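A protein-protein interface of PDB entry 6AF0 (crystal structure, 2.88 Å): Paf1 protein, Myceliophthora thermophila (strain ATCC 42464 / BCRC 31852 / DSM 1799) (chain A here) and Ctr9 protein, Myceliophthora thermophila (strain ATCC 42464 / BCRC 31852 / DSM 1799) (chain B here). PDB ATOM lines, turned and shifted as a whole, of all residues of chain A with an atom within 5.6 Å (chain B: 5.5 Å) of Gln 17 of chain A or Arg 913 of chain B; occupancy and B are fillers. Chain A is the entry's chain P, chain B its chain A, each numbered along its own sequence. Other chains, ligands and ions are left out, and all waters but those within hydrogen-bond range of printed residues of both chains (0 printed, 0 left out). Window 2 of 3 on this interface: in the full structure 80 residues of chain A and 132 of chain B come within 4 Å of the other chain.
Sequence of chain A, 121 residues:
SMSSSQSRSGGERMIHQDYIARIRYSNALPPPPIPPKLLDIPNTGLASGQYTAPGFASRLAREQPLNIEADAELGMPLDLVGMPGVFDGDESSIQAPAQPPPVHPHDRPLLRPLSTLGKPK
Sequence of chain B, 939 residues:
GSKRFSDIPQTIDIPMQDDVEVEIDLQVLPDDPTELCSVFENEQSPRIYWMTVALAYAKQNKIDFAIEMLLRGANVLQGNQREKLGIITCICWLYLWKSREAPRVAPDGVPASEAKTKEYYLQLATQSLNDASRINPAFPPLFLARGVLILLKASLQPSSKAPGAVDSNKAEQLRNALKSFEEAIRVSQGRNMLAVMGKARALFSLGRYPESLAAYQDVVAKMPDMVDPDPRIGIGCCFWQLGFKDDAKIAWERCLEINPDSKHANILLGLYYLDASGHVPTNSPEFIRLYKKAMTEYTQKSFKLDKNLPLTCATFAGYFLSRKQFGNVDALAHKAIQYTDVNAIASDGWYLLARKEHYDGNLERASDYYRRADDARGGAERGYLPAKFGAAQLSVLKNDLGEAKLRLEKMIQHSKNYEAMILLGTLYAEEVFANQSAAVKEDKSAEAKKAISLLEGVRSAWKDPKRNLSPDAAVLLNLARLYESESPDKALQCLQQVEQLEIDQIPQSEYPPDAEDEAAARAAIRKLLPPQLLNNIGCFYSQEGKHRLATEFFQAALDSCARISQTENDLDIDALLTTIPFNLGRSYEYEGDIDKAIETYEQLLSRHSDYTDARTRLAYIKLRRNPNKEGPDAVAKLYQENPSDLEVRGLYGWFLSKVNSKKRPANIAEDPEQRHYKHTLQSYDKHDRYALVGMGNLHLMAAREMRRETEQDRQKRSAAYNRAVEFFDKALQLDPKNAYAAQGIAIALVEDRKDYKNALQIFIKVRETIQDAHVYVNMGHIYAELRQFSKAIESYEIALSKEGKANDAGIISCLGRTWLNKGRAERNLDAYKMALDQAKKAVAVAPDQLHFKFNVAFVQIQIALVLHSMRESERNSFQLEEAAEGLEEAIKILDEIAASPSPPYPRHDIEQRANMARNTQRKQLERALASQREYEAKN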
ATOM      1  N   MET A  14       6.564 -18.776 -29.346  1.00  0.00           N
ATOM      2  CA  MET A  14       7.721 -19.501 -28.758  1.00  0.00           C
ATOM      3  C   MET A  14       8.810 -19.720 -29.799  1.00  0.00           C
ATOM      4  O   MET A  14       9.726 -18.897 -29.933  1.00  0.00           O
ATOM      5  CB  MET A  14       7.300 -20.847 -28.155  1.00  0.00           C
ATOM      6  CG  MET A  14       8.398 -21.924 -28.220  1.00  0.00           C
ATOM      7  SD  MET A  14      10.094 -21.242 -28.270  1.00  0.00           S
ATOM      8  CE  MET A  14      11.105 -22.666 -27.856  1.00  0.00           C
ATOM      9  N   ILE A  15       8.694 -20.823 -30.557  1.00  0.00           N
ATOM     10  CA  ILE A  15       9.779 -21.232 -31.463  1.00  0.00           C
ATOM     11  C   ILE A  15       9.790 -20.334 -32.682  1.00  0.00           C
ATOM     12  O   ILE A  15      10.496 -20.612 -33.663  1.00  0.00           O
ATOM     13  CB  ILE A  15       9.620 -22.678 -31.983  1.00  0.00           C
ATOM     14  CG1 ILE A  15      10.971 -23.403 -31.985  1.00  0.00           C
ATOM     15  CG2 ILE A  15       9.024 -22.679 -33.397  1.00  0.00           C
ATOM     16  CD1 ILE A  15      11.228 -24.226 -33.233  1.00  0.00           C
ATOM     17  N   HIS A  16       8.990 -19.277 -32.647  1.00  0.00           N
ATOM     18  CA  HIS A  16       9.017 -18.326 -33.710  1.00  0.00           C
ATOM     19  C   HIS A  16      10.093 -17.285 -33.512  1.00  0.00           C
ATOM     20  O   HIS A  16      10.228 -16.379 -34.327  1.00  0.00           O
ATOM     21  CB  HIS A  16       7.653 -17.707 -33.837  1.00  0.00           C
ATOM     22  CG  HIS A  16       6.599 -18.712 -34.146  1.00  0.00           C
ATOM     23  ND1 HIS A  16       5.981 -19.457 -33.170  1.00  0.00           N
ATOM     24  CD2 HIS A  16       6.088 -19.132 -35.323  1.00  0.00           C
ATOM     25  CE1 HIS A  16       5.111 -20.274 -33.728  1.00  0.00           C
ATOM     26  NE2 HIS A  16       5.158 -20.102 -35.035  1.00  0.00           N
ATOM     27  N   GLN A  17      10.872 -17.433 -32.444  1.00  0.00           N
ATOM     28  CA  GLN A  17      12.075 -16.637 -32.234  1.00  0.00           C
ATOM     29  C   GLN A  17      13.039 -16.704 -33.394  1.00  0.00           C
ATOM     30  O   GLN A  17      13.166 -17.730 -34.043  1.00  0.00           O
ATOM     31  CB  GLN A  17      12.802 -17.118 -31.003  1.00  0.00           C
ATOM     32  CG  GLN A  17      12.222 -16.549 -29.739  1.00  0.00           C
ATOM     33  CD  GLN A  17      12.634 -17.339 -28.546  1.00  0.00           C
ATOM     34  OE1 GLN A  17      13.682 -17.943 -28.556  1.00  0.00           O
ATOM     35  NE2 GLN A  17      11.804 -17.348 -27.515  1.00  0.00           N
ATOM     36  N   ASP A  18      13.722 -15.594 -33.625  1.00  0.00           N
ATOM     37  CA  ASP A  18      14.638 -15.435 -34.750  1.00  0.00           C
ATOM     38  C   ASP A  18      15.548 -14.256 -34.447  1.00  0.00           C
ATOM     39  O   ASP A  18      15.329 -13.509 -33.498  1.00  0.00           O
ATOM     40  CB  ASP A  18      13.846 -15.169 -36.047  1.00  0.00           C
ATOM     41  CG  ASP A  18      14.656 -15.436 -37.314  1.00  0.00           C
ATOM     42  OD1 ASP A  18      15.907 -15.425 -37.291  1.00  0.00           O
ATOM     43  OD2 ASP A  18      14.019 -15.654 -38.356  1.00  0.00           O
ATOM     44  N   TYR A  19      16.565 -14.080 -35.270  1.00  0.00           N
ATOM     45  CA  TYR A  19      17.399 -12.883 -35.225  1.00  0.00           C
ATOM     46  C   TYR A  19      16.509 -11.650 -35.126  1.00  0.00           C
ATOM     47  O   TYR A  19      15.477 -11.551 -35.788  1.00  0.00           O
ATOM     48  CB  TYR A  19      18.260 -12.817 -36.482  1.00  0.00           C
ATOM     49  CG  TYR A  19      19.537 -12.069 -36.319  1.00  0.00           C
ATOM     50  CD1 TYR A  19      20.733 -12.747 -36.141  1.00  0.00           C
ATOM     51  CD2 TYR A  19      19.566 -10.680 -36.358  1.00  0.00           C
ATOM     52  CE1 TYR A  19      21.927 -12.065 -36.000  1.00  0.00           C
ATOM     53  CE2 TYR A  19      20.758  -9.990 -36.230  1.00  0.00           C
ATOM     54  CZ  TYR A  19      21.932 -10.693 -36.038  1.00  0.00           C
ATOM     55  OH  TYR A  19      23.125 -10.041 -35.896  1.00  0.00           O
ATOM     56  N   PHE B 854      20.876 -11.514 -27.246  1.00  0.00           N
ATOM     57  CA  PHE B 854      20.038 -12.599 -27.769  1.00  0.00           C
ATOM     58  C   PHE B 854      20.499 -13.041 -29.152  1.00  0.00           C
ATOM     59  O   PHE B 854      20.590 -14.223 -29.423  1.00  0.00           O
ATOM     60  CB  PHE B 854      18.582 -12.192 -27.866  1.00  0.00           C
ATOM     61  CG  PHE B 854      17.687 -13.294 -28.341  1.00  0.00           C
ATOM     62  CD1 PHE B 854      16.941 -14.035 -27.444  1.00  0.00           C
ATOM     63  CD2 PHE B 854      17.591 -13.599 -29.688  1.00  0.00           C
ATOM     64  CE1 PHE B 854      16.105 -15.051 -27.883  1.00  0.00           C
ATOM     65  CE2 PHE B 854      16.761 -14.621 -30.131  1.00  0.00           C
ATOM     66  CZ  PHE B 854      16.020 -15.349 -29.227  1.00  0.00           C
ATOM     67  N   PHE B 858      21.332 -16.772 -30.181  1.00  0.00           N
ATOM     68  CA  PHE B 858      20.552 -17.441 -31.230  1.00  0.00           C
ATOM     69  C   PHE B 858      21.473 -17.980 -32.328  1.00  0.00           C
ATOM     70  O   PHE B 858      21.519 -19.176 -32.597  1.00  0.00           O
ATOM     71  CB  PHE B 858      19.544 -16.455 -31.832  1.00  0.00           C
ATOM     72  CG  PHE B 858      18.540 -17.085 -32.757  1.00  0.00           C
ATOM     73  CD1 PHE B 858      17.357 -17.618 -32.268  1.00  0.00           C
ATOM     74  CD2 PHE B 858      18.777 -17.139 -34.117  1.00  0.00           C
ATOM     75  CE1 PHE B 858      16.431 -18.203 -33.123  1.00  0.00           C
ATOM     76  CE2 PHE B 858      17.866 -17.732 -34.975  1.00  0.00           C
ATOM     77  CZ  PHE B 858      16.687 -18.261 -34.478  1.00  0.00           C
ATOM     78  N   ILE B 861      23.473 -20.965 -31.255  1.00  0.00           N
ATOM     79  CA  ILE B 861      22.616 -22.145 -31.177  1.00  0.00           C
ATOM     80  C   ILE B 861      22.331 -22.692 -32.576  1.00  0.00           C
ATOM     81  O   ILE B 861      22.287 -23.898 -32.774  1.00  0.00           O
ATOM     82  CB  ILE B 861      21.309 -21.818 -30.449  1.00  0.00           C
ATOM     83  CG1 ILE B 861      21.627 -21.353 -29.032  1.00  0.00           C
ATOM     84  CG2 ILE B 861      20.414 -23.024 -30.353  1.00  0.00           C
ATOM     85  CD1 ILE B 861      20.413 -20.950 -28.218  1.00  0.00           C
ATOM     86  N   GLN B 862      22.155 -21.815 -33.555  1.00  0.00           N
ATOM     87  CA  GLN B 862      21.923 -22.277 -34.925  1.00  0.00           C
ATOM     88  C   GLN B 862      23.145 -22.975 -35.499  1.00  0.00           C
ATOM     89  O   GLN B 862      23.018 -24.017 -36.108  1.00  0.00           O
ATOM     90  CB  GLN B 862      21.468 -21.134 -35.829  1.00  0.00           C
ATOM     91  CG  GLN B 862      20.155 -20.516 -35.357  1.00  0.00           C
ATOM     92  CD  GLN B 862      19.013 -21.510 -35.323  1.00  0.00           C
ATOM     93  OE1 GLN B 862      18.686 -22.103 -36.343  1.00  0.00           O
ATOM     94  NE2 GLN B 862      18.400 -21.695 -34.147  1.00  0.00           N
ATOM     95  N   LEU B 894      21.714 -16.364 -22.607  1.00  0.00           N
ATOM     96  CA  LEU B 894      20.286 -16.637 -22.452  1.00  0.00           C
ATOM     97  C   LEU B 894      19.865 -16.669 -20.997  1.00  0.00           C
ATOM     98  O   LEU B 894      18.779 -16.210 -20.653  1.00  0.00           O
ATOM     99  CB  LEU B 894      19.905 -17.986 -23.060  1.00  0.00           C
ATOM    100  CG  LEU B 894      19.512 -18.035 -24.533  1.00  0.00           C
ATOM    101  CD1 LEU B 894      20.744 -17.920 -25.391  1.00  0.00           C
ATOM    102  CD2 LEU B 894      18.808 -19.342 -24.847  1.00  0.00           C
ATOM    103  N   TYR B 905      11.746 -11.422 -25.805  1.00  0.00           N
ATOM    104  CA  TYR B 905      10.633 -12.357 -25.801  1.00  0.00           C
ATOM    105  C   TYR B 905      10.297 -12.682 -24.338  1.00  0.00           C
ATOM    106  O   TYR B 905      11.067 -12.334 -23.453  1.00  0.00           O
ATOM    107  CB  TYR B 905      11.032 -13.618 -26.549  1.00  0.00           C
ATOM    108  CG  TYR B 905      11.486 -13.425 -27.988  1.00  0.00           C
ATOM    109  CD1 TYR B 905      10.583 -13.538 -29.048  1.00  0.00           C
ATOM    110  CD2 TYR B 905      12.825 -13.214 -28.292  1.00  0.00           C
ATOM    111  CE1 TYR B 905      11.001 -13.419 -30.361  1.00  0.00           C
ATOM    112  CE2 TYR B 905      13.250 -13.083 -29.603  1.00  0.00           C
ATOM    113  CZ  TYR B 905      12.335 -13.181 -30.628  1.00  0.00           C
ATOM    114  OH  TYR B 905      12.792 -13.052 -31.907  1.00  0.00           O
ATOM    115  N   PRO B 906       9.152 -13.332 -24.075  1.00  0.00           N
ATOM    116  CA  PRO B 906       8.810 -13.771 -22.703  1.00  0.00           C
ATOM    117  C   PRO B 906       9.902 -14.613 -22.065  1.00  0.00           C
ATOM    118  O   PRO B 906      10.433 -15.502 -22.721  1.00  0.00           O
ATOM    119  CB  PRO B 906       7.564 -14.630 -22.907  1.00  0.00           C
ATOM    120  CG  PRO B 906       6.925 -14.082 -24.139  1.00  0.00           C
ATOM    121  CD  PRO B 906       8.006 -13.457 -24.990  1.00  0.00           C
ATOM    122  N   HIS B 908      10.085 -17.068 -20.039  1.00  0.00           N
ATOM    123  CA  HIS B 908       9.867 -18.521 -20.007  1.00  0.00           C
ATOM    124  C   HIS B 908      10.266 -19.186 -21.350  1.00  0.00           C
ATOM    125  O   HIS B 908      10.858 -20.268 -21.369  1.00  0.00           O
ATOM    126  CB  HIS B 908       8.425 -18.859 -19.583  1.00  0.00           C
ATOM    127  CG  HIS B 908       7.473 -19.034 -20.726  1.00  0.00           C
ATOM    128  ND1 HIS B 908       6.974 -20.266 -21.092  1.00  0.00           N
ATOM    129  CD2 HIS B 908       6.934 -18.137 -21.583  1.00  0.00           C
ATOM    130  CE1 HIS B 908       6.163 -20.118 -22.127  1.00  0.00           C
ATOM    131  NE2 HIS B 908       6.125 -18.837 -22.446  1.00  0.00           N
ATOM    132  N   ASP B 909       9.963 -18.517 -22.459  1.00  0.00           N
ATOM    133  CA  ASP B 909      10.389 -18.951 -23.782  1.00  0.00           C
ATOM    134  C   ASP B 909      11.902 -18.917 -23.919  1.00  0.00           C
ATOM    135  O   ASP B 909      12.461 -19.715 -24.663  1.00  0.00           O
ATOM    136  CB  ASP B 909       9.786 -18.055 -24.863  1.00  0.00           C
ATOM    137  CG  ASP B 909       8.354 -18.417 -25.203  1.00  0.00           C
ATOM    138  OD1 ASP B 909       7.703 -19.185 -24.459  1.00  0.00           O
ATOM    139  OD2 ASP B 909       7.879 -17.921 -26.244  1.00  0.00           O
ATOM    140  N   ILE B 910      12.555 -17.981 -23.227  1.00  0.00           N
ATOM    141  CA  ILE B 910      14.016 -17.871 -23.242  1.00  0.00           C
ATOM    142  C   ILE B 910      14.617 -19.032 -22.464  1.00  0.00           C
ATOM    143  O   ILE B 910      15.585 -19.645 -22.902  1.00  0.00           O
ATOM    144  CB  ILE B 910      14.516 -16.516 -22.685  1.00  0.00           C
ATOM    145  CG1 ILE B 910      14.386 -15.417 -23.731  1.00  0.00           C
ATOM    146  CG2 ILE B 910      15.996 -16.559 -22.326  1.00  0.00           C
ATOM    147  CD1 ILE B 910      12.994 -15.236 -24.273  1.00  0.00           C
ATOM    148  N   GLU B 911      14.047 -19.342 -21.311  1.00  0.00           N
ATOM    149  CA  GLU B 911      14.504 -20.520 -20.554  1.00  0.00           C
ATOM    150  C   GLU B 911      14.320 -21.792 -21.372  1.00  0.00           C
ATOM    151  O   GLU B 911      15.208 -22.641 -21.403  1.00  0.00           O
ATOM    152  CB  GLU B 911      13.848 -20.660 -19.172  1.00  0.00           C
ATOM    153  CG  GLU B 911      12.552 -19.907 -18.962  1.00  0.00           C
ATOM    154  CD  GLU B 911      12.387 -19.411 -17.549  1.00  0.00           C
ATOM    155  OE1 GLU B 911      11.294 -19.634 -16.976  1.00  0.00           O
ATOM    156  OE2 GLU B 911      13.353 -18.792 -17.034  1.00  0.00           O
ATOM    157  N   GLN B 912      13.186 -21.903 -22.054  1.00  0.00           N
ATOM    158  CA  GLN B 912      12.931 -23.032 -22.959  1.00  0.00           C
ATOM    159  C   GLN B 912      14.038 -23.214 -23.989  1.00  0.00           C
ATOM    160  O   GLN B 912      14.425 -24.339 -24.305  1.00  0.00           O
ATOM    161  CB  GLN B 912      11.616 -22.832 -23.697  1.00  0.00           C
ATOM    162  CG  GLN B 912      10.391 -22.986 -22.819  1.00  0.00           C
ATOM    163  CD  GLN B 912       9.848 -24.389 -22.826  1.00  0.00           C
ATOM    164  OE1 GLN B 912      10.484 -25.305 -23.338  1.00  0.00           O
ATOM    165  NE2 GLN B 912       8.668 -24.568 -22.244  1.00  0.00           N
ATOM    166  N   ARG B 913      14.520 -22.101 -24.530  1.00  0.00           N
ATOM    167  CA  ARG B 913      15.686 -22.115 -25.423  1.00  0.00           C
ATOM    168  C   ARG B 913      16.953 -22.604 -24.734  1.00  0.00           C
ATOM    169  O   ARG B 913      17.790 -23.266 -25.357  1.00  0.00           O
ATOM    170  CB  ARG B 913      15.973 -20.718 -25.967  1.00  0.00           C
ATOM    171  CG  ARG B 913      15.157 -20.338 -27.176  1.00  0.00           C
ATOM    172  CD  ARG B 913      16.007 -20.283 -28.430  1.00  0.00           C
ATOM    173  NE  ARG B 913      15.133 -20.438 -29.583  1.00  0.00           N
ATOM    174  CZ  ARG B 913      15.517 -20.879 -30.769  1.00  0.00           C
ATOM    175  NH1 ARG B 913      16.789 -21.214 -30.991  1.00  0.00           N
ATOM    176  NH2 ARG B 913      14.616 -20.991 -31.736  1.00  0.00           N
ATOM    177  N   ALA B 914      17.115 -22.229 -23.468  1.00  0.00           N
ATOM    178  CA  ALA B 914      18.273 -22.658 -22.693  1.00  0.00           C
ATOM    179  C   ALA B 914      18.172 -24.135 -22.376  1.00  0.00           C
ATOM    180  O   ALA B 914      19.148 -24.850 -22.486  1.00  0.00           O
ATOM    181  CB  ALA B 914      18.402 -21.845 -21.414  1.00  0.00           C
ATOM    182  N   ASN B 915      16.988 -24.602 -22.003  1.00  0.00           N
ATOM    183  CA  ASN B 915      16.806 -26.028 -21.725  1.00  0.00           C
ATOM    184  C   ASN B 915      17.094 -26.906 -22.932  1.00  0.00           C
ATOM    185  O   ASN B 915      17.715 -27.949 -22.790  1.00  0.00           O
ATOM    186  CB  ASN B 915      15.411 -26.315 -21.159  1.00  0.00           C
ATOM    187  CG  ASN B 915      15.186 -25.679 -19.796  1.00  0.00           C
ATOM    188  OD1 ASN B 915      14.044 -25.495 -19.388  1.00  0.00           O
ATOM    189  ND2 ASN B 915      16.267 -25.340 -19.082  1.00  0.00           N
ATOM    190  N   MET B 916      16.706 -26.471 -24.123  1.00  0.00           N
ATOM    191  CA  MET B 916      17.084 -27.217 -25.293  1.00  0.00           C
ATOM    192  C   MET B 916      18.583 -27.112 -25.530  1.00  0.00           C
ATOM    193  O   MET B 916      19.181 -27.955 -26.188  1.00  0.00           O
ATOM    194  CB  MET B 916      16.329 -26.737 -26.507  1.00  0.00           C
ATOM    195  CG  MET B 916      14.824 -26.848 -26.355  1.00  0.00           C
ATOM    196  SD  MET B 916      14.016 -27.625 -27.767  1.00  0.00           S
ATOM    197  CE  MET B 916      15.091 -27.196 -29.156  1.00  0.00           C
ATOM    198  N   ALA B 917      19.197 -26.081 -24.982  1.00  0.00           N
ATOM    199  CA  ALA B 917      20.640 -25.949 -25.072  1.00  0.00           C
ATOM    200  C   ALA B 917      21.390 -26.964 -24.192  1.00  0.00           C
ATOM    201  O   ALA B 917      22.560 -27.201 -24.427  1.00  0.00           O
ATOM    202  CB  ALA B 917      21.072 -24.529 -24.767  1.00  0.00           C
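Gln 17 of chain A touches Phe 854 of chain B.
Phe 858 of chain B touches Gln 17 of chain A (CE1 to O, 3.4 Å).
Gln 17 of chain A touches Tyr 905 of chain B (CG to CE1, 3.4 Å).
Gln 17 of chain A touches Asp 909 of chain B.
Phe 854 of chain B touches Asp 18 of chain A (CE2 to O, 3.8 Å).
Asp 18 of chain A touches Phe 858 of chain B (CA to CZ, 3.5 Å).
Tyr 19 of chain A touches Phe 858 of chain B.
The side-chain hydroxyl (OH) of Tyr 905 of chain B lies within hydrogen-bond range of the backbone carbonyl oxygen (O) of Asp 18 of chain A (3.0 Å).
The side-chain carboxylate (OD2) of Asp 909 of chain B lies close to the backbone NH (N) of Met 14 of chain A, at 3.5 Å.
The side-chain amide oxygen (OE1) of Gln 17 of chain A lies within hydrogen-bond range of the guanidinium group (NE) of Arg 913 of chain B (3.1 Å).
A ring nitrogen (NE2) of His 908 of chain B is in hydrogen-bond range of the side-chain carboxylate of Asp 909 of chain B (2.6 Å).
Printed residues of chain A that touch a printed residue of chain B: Met 14, Gln 17, Asp 18 and Tyr 19.
Hydrophobic or aromatic side chains of chain A within 4 Å of the printed part of chain B: Met 14.
Of the 17 printed residues of chain B, 5 touch a printed residue of chain A.
Printed residues of chain B that touch a printed residue of chain A: Phe 854, Phe 858, Tyr 905, Asp 909 and Arg 913.
Hydrophobic or aromatic side chains of chain B within 4 Å of the printed part of chain A: Phe 854, Phe 858 and Tyr 905.
Along chain B the printed residues that touch a printed residue of chain A span positions 854 to 913.
Among the printed residues, no Asp or Glu carboxylate lies within 4 Å of a Lys or Arg side-chain nitrogen of the other chain.
Gln 17 of chain A touches five residues of chain B.
Arg 913 of chain B touches just one residue of chain A: Gln 17 (3.1 Å).
Printed residues of chain A within 4 Å of Phe 854 of chain B: Gln 17 and Asp 18.
Of the printed residues of chain A, Phe 858 of chain B touches Gln 17 (3.4 Å), Asp 18 (3.5 Å) and Tyr 19 (3.9 Å).
Printed residues of chain B within 4 Å of Tyr 19 of chain A: Phe 858.
Of the printed residues of chain A, Asp 909 of chain B touches Met 14 and Gln 17.
The nearest residue of chain B that does not touch Gln 17 of chain A is Ile 910 of chain B (4.05 Å).
The nearest residue of chain A that does not touch Arg 913 of chain B is Ile 15 of chain A (4.4 Å).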
